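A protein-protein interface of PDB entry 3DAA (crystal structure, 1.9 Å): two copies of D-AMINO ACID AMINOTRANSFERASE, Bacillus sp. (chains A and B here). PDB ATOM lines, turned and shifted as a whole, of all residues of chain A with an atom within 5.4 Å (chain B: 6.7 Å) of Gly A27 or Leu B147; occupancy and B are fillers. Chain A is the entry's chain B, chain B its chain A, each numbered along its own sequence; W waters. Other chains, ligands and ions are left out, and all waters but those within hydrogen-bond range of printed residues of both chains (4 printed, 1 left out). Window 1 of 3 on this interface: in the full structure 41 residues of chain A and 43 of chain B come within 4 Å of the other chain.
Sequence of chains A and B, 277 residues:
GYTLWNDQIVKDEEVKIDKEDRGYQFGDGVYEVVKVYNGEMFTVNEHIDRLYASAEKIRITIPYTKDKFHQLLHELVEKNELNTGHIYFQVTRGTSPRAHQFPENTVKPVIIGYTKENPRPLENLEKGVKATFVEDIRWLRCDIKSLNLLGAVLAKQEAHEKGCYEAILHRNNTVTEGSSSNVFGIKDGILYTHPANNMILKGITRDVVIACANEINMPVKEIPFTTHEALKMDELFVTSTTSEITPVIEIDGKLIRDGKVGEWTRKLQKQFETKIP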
ATOM      1  N   ARG A  22      10.095   8.267  12.921  1.00  0.00           N
ATOM      2  CA  ARG A  22      10.132   9.467  12.080  1.00  0.00           C
ATOM      3  C   ARG A  22      10.274  10.809  12.809  1.00  0.00           C
ATOM      4  O   ARG A  22      10.660  11.812  12.208  1.00  0.00           O
ATOM      5  CB  ARG A  22       8.947   9.456  11.100  1.00  0.00           C
ATOM      6  CG  ARG A  22       9.008   8.272  10.122  1.00  0.00           C
ATOM      7  CD  ARG A  22       7.717   8.084   9.327  1.00  0.00           C
ATOM      8  NE  ARG A  22       7.428   9.207   8.432  1.00  0.00           N
ATOM      9  CZ  ARG A  22       7.885   9.322   7.187  1.00  0.00           C
ATOM     10  NH1 ARG A  22       8.667   8.381   6.662  1.00  0.00           N
ATOM     11  NH2 ARG A  22       7.560  10.388   6.466  1.00  0.00           N
ATOM     12  N   GLY A  23      10.008  10.820  14.109  1.00  0.00           N
ATOM     13  CA  GLY A  23      10.165  12.049  14.870  1.00  0.00           C
ATOM     14  C   GLY A  23      11.647  12.294  15.135  1.00  0.00           C
ATOM     15  O   GLY A  23      12.066  13.428  15.391  1.00  0.00           O
ATOM     16  N   TYR A  24      12.439  11.222  15.036  1.00  0.00           N
ATOM     17  CA  TYR A  24      13.882  11.274  15.267  1.00  0.00           C
ATOM     18  C   TYR A  24      14.690  11.539  13.992  1.00  0.00           C
ATOM     19  O   TYR A  24      15.742  12.188  14.032  1.00  0.00           O
ATOM     20  CB  TYR A  24      14.347   9.964  15.907  1.00  0.00           C
ATOM     21  CG  TYR A  24      15.726  10.016  16.523  1.00  0.00           C
ATOM     22  CD1 TYR A  24      16.033  10.949  17.514  1.00  0.00           C
ATOM     23  CD2 TYR A  24      16.714   9.103  16.151  1.00  0.00           C
ATOM     24  CE1 TYR A  24      17.286  10.973  18.121  1.00  0.00           C
ATOM     25  CE2 TYR A  24      17.980   9.114  16.758  1.00  0.00           C
ATOM     26  CZ  TYR A  24      18.256  10.053  17.743  1.00  0.00           C
ATOM     27  OH  TYR A  24      19.491  10.073  18.350  1.00  0.00           O
ATOM     28  N   GLN A  25      14.195  11.047  12.862  1.00  0.00           N
ATOM     29  CA  GLN A  25      14.900  11.226  11.597  1.00  0.00           C
ATOM     30  C   GLN A  25      14.444  12.411  10.739  1.00  0.00           C
ATOM     31  O   GLN A  25      15.228  12.927   9.941  1.00  0.00           O
ATOM     32  CB  GLN A  25      14.846   9.933  10.782  1.00  0.00           C
ATOM     33  CG  GLN A  25      15.562   8.760  11.427  1.00  0.00           C
ATOM     34  CD  GLN A  25      15.746   7.592  10.471  1.00  0.00           C
ATOM     35  OE1 GLN A  25      14.786   7.121   9.855  1.00  0.00           O
ATOM     36  NE2 GLN A  25      16.982   7.117  10.340  1.00  0.00           N
ATOM     37  N   PHE A  26      13.200  12.857  10.918  1.00  0.00           N
ATOM     38  CA  PHE A  26      12.659  13.969  10.128  1.00  0.00           C
ATOM     39  C   PHE A  26      11.958  15.047  10.958  1.00  0.00           C
ATOM     40  O   PHE A  26      11.535  16.071  10.411  1.00  0.00           O
ATOM     41  CB  PHE A  26      11.637  13.457   9.103  1.00  0.00           C
ATOM     42  CG  PHE A  26      12.150  12.368   8.204  1.00  0.00           C
ATOM     43  CD1 PHE A  26      12.851  12.676   7.045  1.00  0.00           C
ATOM     44  CD2 PHE A  26      11.890  11.033   8.493  1.00  0.00           C
ATOM     45  CE1 PHE A  26      13.284  11.670   6.186  1.00  0.00           C
ATOM     46  CE2 PHE A  26      12.315  10.016   7.644  1.00  0.00           C
ATOM     47  CZ  PHE A  26      13.014  10.336   6.484  1.00  0.00           C
ATOM     48  N   GLY A  27      11.828  14.822  12.266  1.00  0.00           N
ATOM     49  CA  GLY A  27      11.116  15.774  13.111  1.00  0.00           C
ATOM     50  C   GLY A  27       9.659  15.726  12.670  1.00  0.00           C
ATOM     51  O   GLY A  27       8.927  16.709  12.762  1.00  0.00           O
ATOM     52  N   ASP A  28       9.275  14.570  12.128  1.00  0.00           N
ATOM     53  CA  ASP A  28       7.932  14.296  11.619  1.00  0.00           C
ATOM     54  C   ASP A  28       6.971  14.023  12.787  1.00  0.00           C
ATOM     55  O   ASP A  28       6.653  12.872  13.094  1.00  0.00           O
ATOM     56  CB  ASP A  28       8.011  13.086  10.656  1.00  0.00           C
ATOM     57  CG  ASP A  28       6.718  12.826   9.896  1.00  0.00           C
ATOM     58  OD1 ASP A  28       5.742  13.602  10.028  1.00  0.00           O
ATOM     59  OD2 ASP A  28       6.682  11.822   9.152  1.00  0.00           O
ATOM     60  N   GLY A  29       6.524  15.099  13.434  1.00  0.00           N
ATOM     61  CA  GLY A  29       5.609  14.990  14.560  1.00  0.00           C
ATOM     62  C   GLY A  29       5.180  16.341  15.114  1.00  0.00           C
ATOM     63  O   GLY A  29       5.678  17.384  14.693  1.00  0.00           O
ATOM     64  N   SER A 146       5.056  21.795  15.223  1.00  0.00           N
ATOM     65  CA  SER A 146       5.889  20.634  14.923  1.00  0.00           C
ATOM     66  C   SER A 146       7.212  20.554  15.664  1.00  0.00           C
ATOM     67  O   SER A 146       7.669  21.530  16.271  1.00  0.00           O
ATOM     68  CB  SER A 146       6.162  20.548  13.416  1.00  0.00           C
ATOM     69  OG  SER A 146       7.233  21.395  13.033  1.00  0.00           O
ATOM     70  N   LEU A 147       7.848  19.389  15.539  1.00  0.00           N
ATOM     71  CA  LEU A 147       9.134  19.096  16.167  1.00  0.00           C
ATOM     72  C   LEU A 147      10.314  19.689  15.400  1.00  0.00           C
ATOM     73  O   LEU A 147      11.469  19.510  15.792  1.00  0.00           O
ATOM     74  CB  LEU A 147       9.310  17.580  16.341  1.00  0.00           C
ATOM     75  CG  LEU A 147       8.325  16.865  17.282  1.00  0.00           C
ATOM     76  CD1 LEU A 147       8.412  15.363  17.092  1.00  0.00           C
ATOM     77  CD2 LEU A 147       8.586  17.240  18.737  1.00  0.00           C
ATOM     78  N   ASN A 148      10.029  20.349  14.279  1.00  0.00           N
ATOM     79  CA  ASN A 148      11.062  21.007  13.481  1.00  0.00           C
ATOM     80  C   ASN A 148      11.292  22.332  14.192  1.00  0.00           C
ATOM     81  O   ASN A 148      10.642  23.336  13.887  1.00  0.00           O
ATOM     82  CB  ASN A 148      10.563  21.248  12.050  1.00  0.00           C
ATOM     83  CG  ASN A 148      10.822  20.062  11.134  1.00  0.00           C
ATOM     84  OD1 ASN A 148      11.172  20.237   9.967  1.00  0.00           O
ATOM     85  ND2 ASN A 148      10.690  18.851  11.670  1.00  0.00           N
ATOM     86  N   ARG B  22      17.715  15.568  21.962  1.00  0.00           N
ATOM     87  CA  ARG B  22      17.334  16.799  21.259  1.00  0.00           C
ATOM     88  C   ARG B  22      16.989  16.583  19.789  1.00  0.00           C
ATOM     89  O   ARG B  22      16.352  17.435  19.173  1.00  0.00           O
ATOM     90  CB  ARG B  22      18.411  17.879  21.429  1.00  0.00           C
ATOM     91  CG  ARG B  22      18.495  18.398  22.865  1.00  0.00           C
ATOM     92  CD  ARG B  22      19.653  19.356  23.086  1.00  0.00           C
ATOM     93  NE  ARG B  22      19.537  20.587  22.301  1.00  0.00           N
ATOM     94  CZ  ARG B  22      18.986  21.719  22.734  1.00  0.00           C
ATOM     95  NH1 ARG B  22      18.480  21.789  23.958  1.00  0.00           N
ATOM     96  NH2 ARG B  22      18.988  22.800  21.955  1.00  0.00           N
ATOM     97  N   GLY B  23      17.403  15.441  19.237  1.00  0.00           N
ATOM     98  CA  GLY B  23      17.090  15.120  17.855  1.00  0.00           C
ATOM     99  C   GLY B  23      15.644  14.664  17.752  1.00  0.00           C
ATOM    100  O   GLY B  23      15.027  14.733  16.693  1.00  0.00           O
ATOM    101  N   TYR B  24      15.089  14.226  18.876  1.00  0.00           N
ATOM    102  CA  TYR B  24      13.712  13.754  18.928  1.00  0.00           C
ATOM    103  C   TYR B  24      12.726  14.869  19.315  1.00  0.00           C
ATOM    104  O   TYR B  24      11.546  14.816  18.953  1.00  0.00           O
ATOM    105  CB  TYR B  24      13.622  12.581  19.912  1.00  0.00           C
ATOM    106  CG  TYR B  24      12.364  11.752  19.810  1.00  0.00           C
ATOM    107  CD1 TYR B  24      11.995  11.146  18.608  1.00  0.00           C
ATOM    108  CD2 TYR B  24      11.564  11.530  20.931  1.00  0.00           C
ATOM    109  CE1 TYR B  24      10.863  10.337  18.530  1.00  0.00           C
ATOM    110  CE2 TYR B  24      10.437  10.728  20.864  1.00  0.00           C
ATOM    111  CZ  TYR B  24      10.091  10.133  19.666  1.00  0.00           C
ATOM    112  OH  TYR B  24       8.974   9.337  19.608  1.00  0.00           O
ATOM    113  N   PHE B  26      13.627  18.432  19.006  1.00  0.00           N
ATOM    114  CA  PHE B  26      13.903  19.645  18.235  1.00  0.00           C
ATOM    115  C   PHE B  26      14.425  19.385  16.825  1.00  0.00           C
ATOM    116  O   PHE B  26      14.518  20.317  16.017  1.00  0.00           O
ATOM    117  CB  PHE B  26      14.945  20.507  18.972  1.00  0.00           C
ATOM    118  CG  PHE B  26      14.536  20.923  20.371  1.00  0.00           C
ATOM    119  CD1 PHE B  26      13.689  22.017  20.574  1.00  0.00           C
ATOM    120  CD2 PHE B  26      15.009  20.226  21.485  1.00  0.00           C
ATOM    121  CE1 PHE B  26      13.317  22.416  21.874  1.00  0.00           C
ATOM    122  CE2 PHE B  26      14.647  20.612  22.788  1.00  0.00           C
ATOM    123  CZ  PHE B  26      13.799  21.711  22.981  1.00  0.00           C
ATOM    124  N   GLY B  27      14.758  18.130  16.523  1.00  0.00           N
ATOM    125  CA  GLY B  27      15.324  17.812  15.220  1.00  0.00           C
ATOM    126  C   GLY B  27      16.692  18.477  15.184  1.00  0.00           C
ATOM    127  O   GLY B  27      17.220  18.810  14.119  1.00  0.00           O
ATOM    128  N   ASP B  28      17.258  18.658  16.379  1.00  0.00           N
ATOM    129  CA  ASP B  28      18.554  19.308  16.605  1.00  0.00           C
ATOM    130  C   ASP B  28      19.709  18.353  16.305  1.00  0.00           C
ATOM    131  O   ASP B  28      20.352  17.812  17.212  1.00  0.00           O
ATOM    132  CB  ASP B  28      18.600  19.798  18.070  1.00  0.00           C
ATOM    133  CG  ASP B  28      19.756  20.736  18.355  1.00  0.00           C
ATOM    134  OD1 ASP B  28      20.500  21.114  17.423  1.00  0.00           O
ATOM    135  OD2 ASP B  28      19.905  21.113  19.535  1.00  0.00           O
ATOM    136  N   GLY B  29      19.982  18.168  15.021  1.00  0.00           N
ATOM    137  CA  GLY B  29      21.049  17.277  14.603  1.00  0.00           C
ATOM    138  C   GLY B  29      21.244  17.348  13.101  1.00  0.00           C
ATOM    139  O   GLY B  29      20.412  17.911  12.394  1.00  0.00           O
ATOM    140  N   VAL B  30      22.336  16.765  12.618  1.00  0.00           N
ATOM    141  CA  VAL B  30      22.669  16.767  11.199  1.00  0.00           C
ATOM    142  C   VAL B  30      22.907  15.331  10.736  1.00  0.00           C
ATOM    143  O   VAL B  30      23.129  14.450  11.569  1.00  0.00           O
ATOM    144  CB  VAL B  30      23.915  17.639  10.946  1.00  0.00           C
ATOM    145  CG1 VAL B  30      23.661  19.042  11.455  1.00  0.00           C
ATOM    146  CG2 VAL B  30      25.138  17.060  11.648  1.00  0.00           C
ATOM    147  N   TYR B  31      22.879  15.085   9.426  1.00  0.00           N
ATOM    148  CA  TYR B  31      23.060  13.717   8.931  1.00  0.00           C
ATOM    149  C   TYR B  31      23.733  13.596   7.566  1.00  0.00           C
ATOM    150  O   TYR B  31      23.948  14.588   6.876  1.00  0.00           O
ATOM    151  CB  TYR B  31      21.702  12.996   8.878  1.00  0.00           C
ATOM    152  CG  TYR B  31      20.832  13.407   7.709  1.00  0.00           C
ATOM    153  CD1 TYR B  31      20.110  14.595   7.738  1.00  0.00           C
ATOM    154  CD2 TYR B  31      20.751  12.612   6.559  1.00  0.00           C
ATOM    155  CE1 TYR B  31      19.325  14.990   6.654  1.00  0.00           C
ATOM    156  CE2 TYR B  31      19.969  12.995   5.467  1.00  0.00           C
ATOM    157  CZ  TYR B  31      19.259  14.185   5.523  1.00  0.00           C
ATOM    158  OH  TYR B  31      18.479  14.570   4.454  1.00  0.00           O
ATOM    159  N   TYR B  88      23.641   5.170   6.356  1.00  0.00           N
ATOM    160  CA  TYR B  88      22.995   6.380   6.859  1.00  0.00           C
ATOM    161  C   TYR B  88      23.570   6.659   8.235  1.00  0.00           C
ATOM    162  O   TYR B  88      23.650   5.752   9.059  1.00  0.00           O
ATOM    163  CB  TYR B  88      21.478   6.196   6.999  1.00  0.00           C
ATOM    164  CG  TYR B  88      20.794   7.360   7.701  1.00  0.00           C
ATOM    165  CD1 TYR B  88      20.442   8.516   6.998  1.00  0.00           C
ATOM    166  CD2 TYR B  88      20.578   7.341   9.081  1.00  0.00           C
ATOM    167  CE1 TYR B  88      19.906   9.629   7.649  1.00  0.00           C
ATOM    168  CE2 TYR B  88      20.040   8.452   9.750  1.00  0.00           C
ATOM    169  CZ  TYR B  88      19.712   9.594   9.022  1.00  0.00           C
ATOM    170  OH  TYR B  88      19.216  10.703   9.670  1.00  0.00           O
ATOM    171  N   GLN B  90      23.877   9.831  11.536  1.00  0.00           N
ATOM    172  CA  GLN B  90      23.494  11.125  12.089  1.00  0.00           C
ATOM    173  C   GLN B  90      24.073  11.380  13.483  1.00  0.00           C
ATOM    174  O   GLN B  90      24.476  10.453  14.197  1.00  0.00           O
ATOM    175  CB  GLN B  90      21.964  11.244  12.154  1.00  0.00           C
ATOM    176  CG  GLN B  90      21.297  10.226  13.079  1.00  0.00           C
ATOM    177  CD  GLN B  90      19.836  10.524  13.341  1.00  0.00           C
ATOM    178  OE1 GLN B  90      18.987  10.372  12.465  1.00  0.00           O
ATOM    179  NE2 GLN B  90      19.527  10.919  14.568  1.00  0.00           N
ATOM    180  N   VAL B  91      24.080  12.653  13.864  1.00  0.00           N
ATOM    181  CA  VAL B  91      24.576  13.076  15.164  1.00  0.00           C
ATOM    182  C   VAL B  91      23.673  14.213  15.667  1.00  0.00           C
ATOM    183  O   VAL B  91      23.331  15.126  14.909  1.00  0.00           O
ATOM    184  CB  VAL B  91      26.097  13.494  15.083  1.00  0.00           C
ATOM    185  CG1 VAL B  91      26.299  14.631  14.102  1.00  0.00           C
ATOM    186  CG2 VAL B  91      26.639  13.868  16.463  1.00  0.00           C
ATOM    187  N   THR B  92      23.171  14.070  16.893  1.00  0.00           N
ATOM    188  CA  THR B  92      22.315  15.089  17.504  1.00  0.00           C
ATOM    189  C   THR B  92      23.124  15.784  18.600  1.00  0.00           C
ATOM    190  O   THR B  92      24.211  15.323  18.951  1.00  0.00           O
ATOM    191  CB  THR B  92      21.060  14.460  18.149  1.00  0.00           C
ATOM    192  OG1 THR B  92      21.436  13.724  19.320  1.00  0.00           O
ATOM    193  CG2 THR B  92      20.385  13.518  17.182  1.00  0.00           C
ATOM    194  N   ILE B 144      22.535  23.712   5.585  1.00  0.00           N
ATOM    195  CA  ILE B 144      22.811  22.800   6.699  1.00  0.00           C
ATOM    196  C   ILE B 144      21.950  21.558   6.464  1.00  0.00           C
ATOM    197  O   ILE B 144      20.735  21.676   6.265  1.00  0.00           O
ATOM    198  CB  ILE B 144      22.365  23.411   8.052  1.00  0.00           C
ATOM    199  CG1 ILE B 144      23.015  24.775   8.267  1.00  0.00           C
ATOM    200  CG2 ILE B 144      22.715  22.476   9.212  1.00  0.00           C
ATOM    201  CD1 ILE B 144      22.500  25.492   9.493  1.00  0.00           C
ATOM    202  N   LYS B 145      22.577  20.378   6.463  1.00  0.00           N
ATOM    203  CA  LYS B 145      21.859  19.111   6.254  1.00  0.00           C
ATOM    204  C   LYS B 145      21.342  18.626   7.611  1.00  0.00           C
ATOM    205  O   LYS B 145      21.871  17.674   8.194  1.00  0.00           O
ATOM    206  CB  LYS B 145      22.798  18.074   5.620  1.00  0.00           C
ATOM    207  CG  LYS B 145      22.106  16.880   4.938  1.00  0.00           C
ATOM    208  CD  LYS B 145      23.123  16.046   4.131  1.00  0.00           C
ATOM    209  CE  LYS B 145      22.530  14.774   3.545  1.00  0.00           C
ATOM    210  NZ  LYS B 145      21.422  15.040   2.597  1.00  0.00           N
ATOM    211  N   SER B 146      20.316  19.310   8.110  1.00  0.00           N
ATOM    212  CA  SER B 146      19.722  19.007   9.408  1.00  0.00           C
ATOM    213  C   SER B 146      18.563  18.007   9.378  1.00  0.00           C
ATOM    214  O   SER B 146      18.049  17.663   8.316  1.00  0.00           O
ATOM    215  CB  SER B 146      19.244  20.298  10.069  1.00  0.00           C
ATOM    216  OG  SER B 146      17.990  20.700   9.543  1.00  0.00           O
ATOM    217  N   LEU B 147      18.149  17.579  10.571  1.00  0.00           N
ATOM    218  CA  LEU B 147      17.044  16.638  10.749  1.00  0.00           C
ATOM    219  C   LEU B 147      15.661  17.287  10.624  1.00  0.00           C
ATOM    220  O   LEU B 147      14.648  16.588  10.700  1.00  0.00           O
ATOM    221  CB  LEU B 147      17.167  15.918  12.099  1.00  0.00           C
ATOM    222  CG  LEU B 147      18.399  15.026  12.276  1.00  0.00           C
ATOM    223  CD1 LEU B 147      18.429  14.455  13.682  1.00  0.00           C
ATOM    224  CD2 LEU B 147      18.385  13.920  11.239  1.00  0.00           C
ATOM    225  N   ASN B 148      15.617  18.617  10.486  1.00  0.00           N
ATOM    226  CA  ASN B 148      14.350  19.340  10.301  1.00  0.00           C
ATOM    227  C   ASN B 148      13.984  19.098   8.835  1.00  0.00           C
ATOM    228  O   ASN B 148      14.301  19.911   7.968  1.00  0.00           O
ATOM    229  CB  ASN B 148      14.521  20.854  10.538  1.00  0.00           C
ATOM    230  CG  ASN B 148      14.436  21.242  12.010  1.00  0.00           C
ATOM    231  OD1 ASN B 148      13.901  22.300  12.350  1.00  0.00           O
ATOM    232  ND2 ASN B 148      14.970  20.400  12.884  1.00  0.00           N
ATOM    233  N   LEU B 149      13.295  17.991   8.571  1.00  0.00           N
ATOM    234  CA  LEU B 149      12.935  17.610   7.212  1.00  0.00           C
ATOM    235  C   LEU B 149      11.435  17.496   6.914  1.00  0.00           C
ATOM    236  O   LEU B 149      11.046  16.889   5.903  1.00  0.00           O
ATOM    237  CB  LEU B 149      13.614  16.278   6.884  1.00  0.00           C
ATOM    238  CG  LEU B 149      15.144  16.246   6.910  1.00  0.00           C
ATOM    239  CD1 LEU B 149      15.642  14.815   6.795  1.00  0.00           C
ATOM    240  CD2 LEU B 149      15.689  17.103   5.779  1.00  0.00           C
ATOM    241  N   LEU B 150      10.600  18.096   7.760  1.00  0.00           N
ATOM    242  CA  LEU B 150       9.150  18.024   7.578  1.00  0.00           C
ATOM    243  C   LEU B 150       8.667  18.591   6.241  1.00  0.00           C
ATOM    244  O   LEU B 150       7.757  18.029   5.619  1.00  0.00           O
ATOM    245  CB  LEU B 150       8.420  18.685   8.753  1.00  0.00           C
ATOM    246  CG  LEU B 150       6.914  18.422   8.850  1.00  0.00           C
ATOM    247  CD1 LEU B 150       6.602  16.936   8.702  1.00  0.00           C
ATOM    248  CD2 LEU B 150       6.389  18.960  10.169  1.00  0.00           C
HETATM  249  O   HOH W   1      10.737  21.349   7.390  1.00  0.00           O
HETATM  250  O   HOH W   2      17.078  11.537   8.147  1.00  0.00           O
HETATM  251  O   HOH W   3      21.799  10.277  16.605  1.00  0.00           O
HETATM  252  O   HOH W   4      18.350   7.427  13.131  1.00  0.00           O
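O of Gly B23 sits close to O of Gly A23 (3.5 Å). The backbone carbonyl oxygen (O) of Phe A26 lies within hydrogen-bond range of the backbone NH (N) of Leu B149 (3.2 Å). The backbone carbonyl oxygen of Phe A26 sits at hydrogen-bond distance from the backbone NH of Leu B150, 3.5 Å away. The side-chain amide oxygen (OD1) of Asn A148 is in hydrogen-bond range of the backbone NH (N) of Leu B149 (3.4 Å). The backbone carbonyl oxygen of Phe A26 sits close to the backbone carbonyl oxygen of Leu B147 (3.2 Å). O of Phe B26 sits close to O of Leu A147, 3.2 Å away. N of Leu B150 lies within hydrogen-bond range of OD1 of Asn A148, at 3.1 Å.
The side-chain amide nitrogen of Asn A148 sits at hydrogen-bond distance from the backbone carbonyl oxygen of Gly A27, 3.0 Å away. The backbone carbonyl oxygen (O) of Gly B27 is in hydrogen-bond range of the side-chain amide nitrogen (ND2) of Asn B148, 3.0 Å away. The side-chain hydroxyl (OH) of Tyr B88 lies within hydrogen-bond range of the side-chain amide oxygen (OE1) of Gln B90 (2.8 Å). The backbone carbonyl oxygen (O) of Arg A22 sits at hydrogen-bond distance from the backbone NH (N) of Gly A27 (3.2 Å). O of Phe B26 lies within hydrogen-bond range of ND2 of Asn B148. OD2 of Asp A28 lies within salt-bridge range of NE of Arg A22 (2.8 Å).
C of Gly A23 touches CD1 of Tyr B24, at 3.7 Å. CE2 of Tyr A24 touches NE2 of Gln B90, at 3.2 Å. Thr B92 touches Tyr A24 (CG2 to OH, 3.7 Å). CD1 of Leu B147 touches O of Tyr A24, 3.5 Å away. Tyr B88 touches Gln A25 (CE2 to NE2, 3.4 Å). Gln A25 touches Gln B90 (CG to OE1, 3.9 Å). Leu B147 touches Gln A25 (CD2 to O, 3.6 Å). Gly A27 touches Leu B147 (N to O, 3.7 Å). OD1 of Asp A28 touches CD1 of Leu B150 (3.7 Å). Asn B148 touches Asn A148 (OD1 to C, 3.2 Å).
Of the printed residues of chain B, Tyr A24 touches Gly B23 (3.7 Å), Tyr B24 (3.6 Å), Gln B90 (3.2 Å), Thr B92 (3.7 Å) and Leu B147 (3.5 Å). Of the printed residues of chain B, Gly A27 touches Leu B147 (3.7 Å). Arg B22 touches none of the printed residues of chain A. Printed residues of chain A within 4 Å of Tyr B24: Gly A23, Tyr A24 and Leu A147. Gly B29 touches none of the printed residues of chain A. Of the printed residues of chain A, Tyr B88 touches Gln A25 (3.4 Å). Of the printed residues of chain A, Gln B90 touches Tyr A24 (3.2 Å) and Gln A25 (3.9 Å). Leu B147 touches just these residues of chain A: Tyr A24, Gln A25, Phe A26 and Gly A27. The nearest residue of chain B that does not touch Gly A27 is Leu B150 (4.3 Å). The nearest residue of chain A that does not touch Leu B147 is Asn A148 (4.7 Å).
Printed residues of chain A that touch a printed residue of chain B: Gly A23, Tyr A24, Gln A25, Phe A26, Gly A27, Asp A28, Ser A146, Leu A147 and Asn A148. Hydrophobic or aromatic side chains of chain A within 4 Å of the printed part of chain B: Tyr A24, Phe A26 and Leu A147. Of the 20 printed residues of chain B, 11 touch a printed residue of chain A. Hydrophobic or aromatic side chains of chain B that line the printed part of chain A: Tyr B24, Tyr B88, Leu B147, Leu B149 and Leu B150.
Gly A23 touches Tyr B24, and with the chains exchanged Tyr A24 touches Gly B23. Tyr A24 touches its own counterpart, Tyr B24. Gly A27 touches Leu B147, and with the chains exchanged Leu A147 touches Gly B27. Asn A148 touches its own counterpart, Asn B148.
Water W2 lies within hydrogen-bond range of OH of Tyr B88 (2.8 Å) and O of Gln A25 (2.9 Å). Water W1 lies within hydrogen-bond range of the side-chain amide oxygen of Asn A148 (2.8 Å) and the backbone NH of Leu B150 (3.3 Å). Water W3 lies within hydrogen-bond range of the side-chain hydroxyl of Tyr A24 and the side-chain amide nitrogen of Gln B90. Water W4 bridges the side-chain amide oxygen (OE1) of Gln B90 (3.1 Å) and the side-chain amide nitrogen (NE2) of Gln A25 (3.1 Å).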
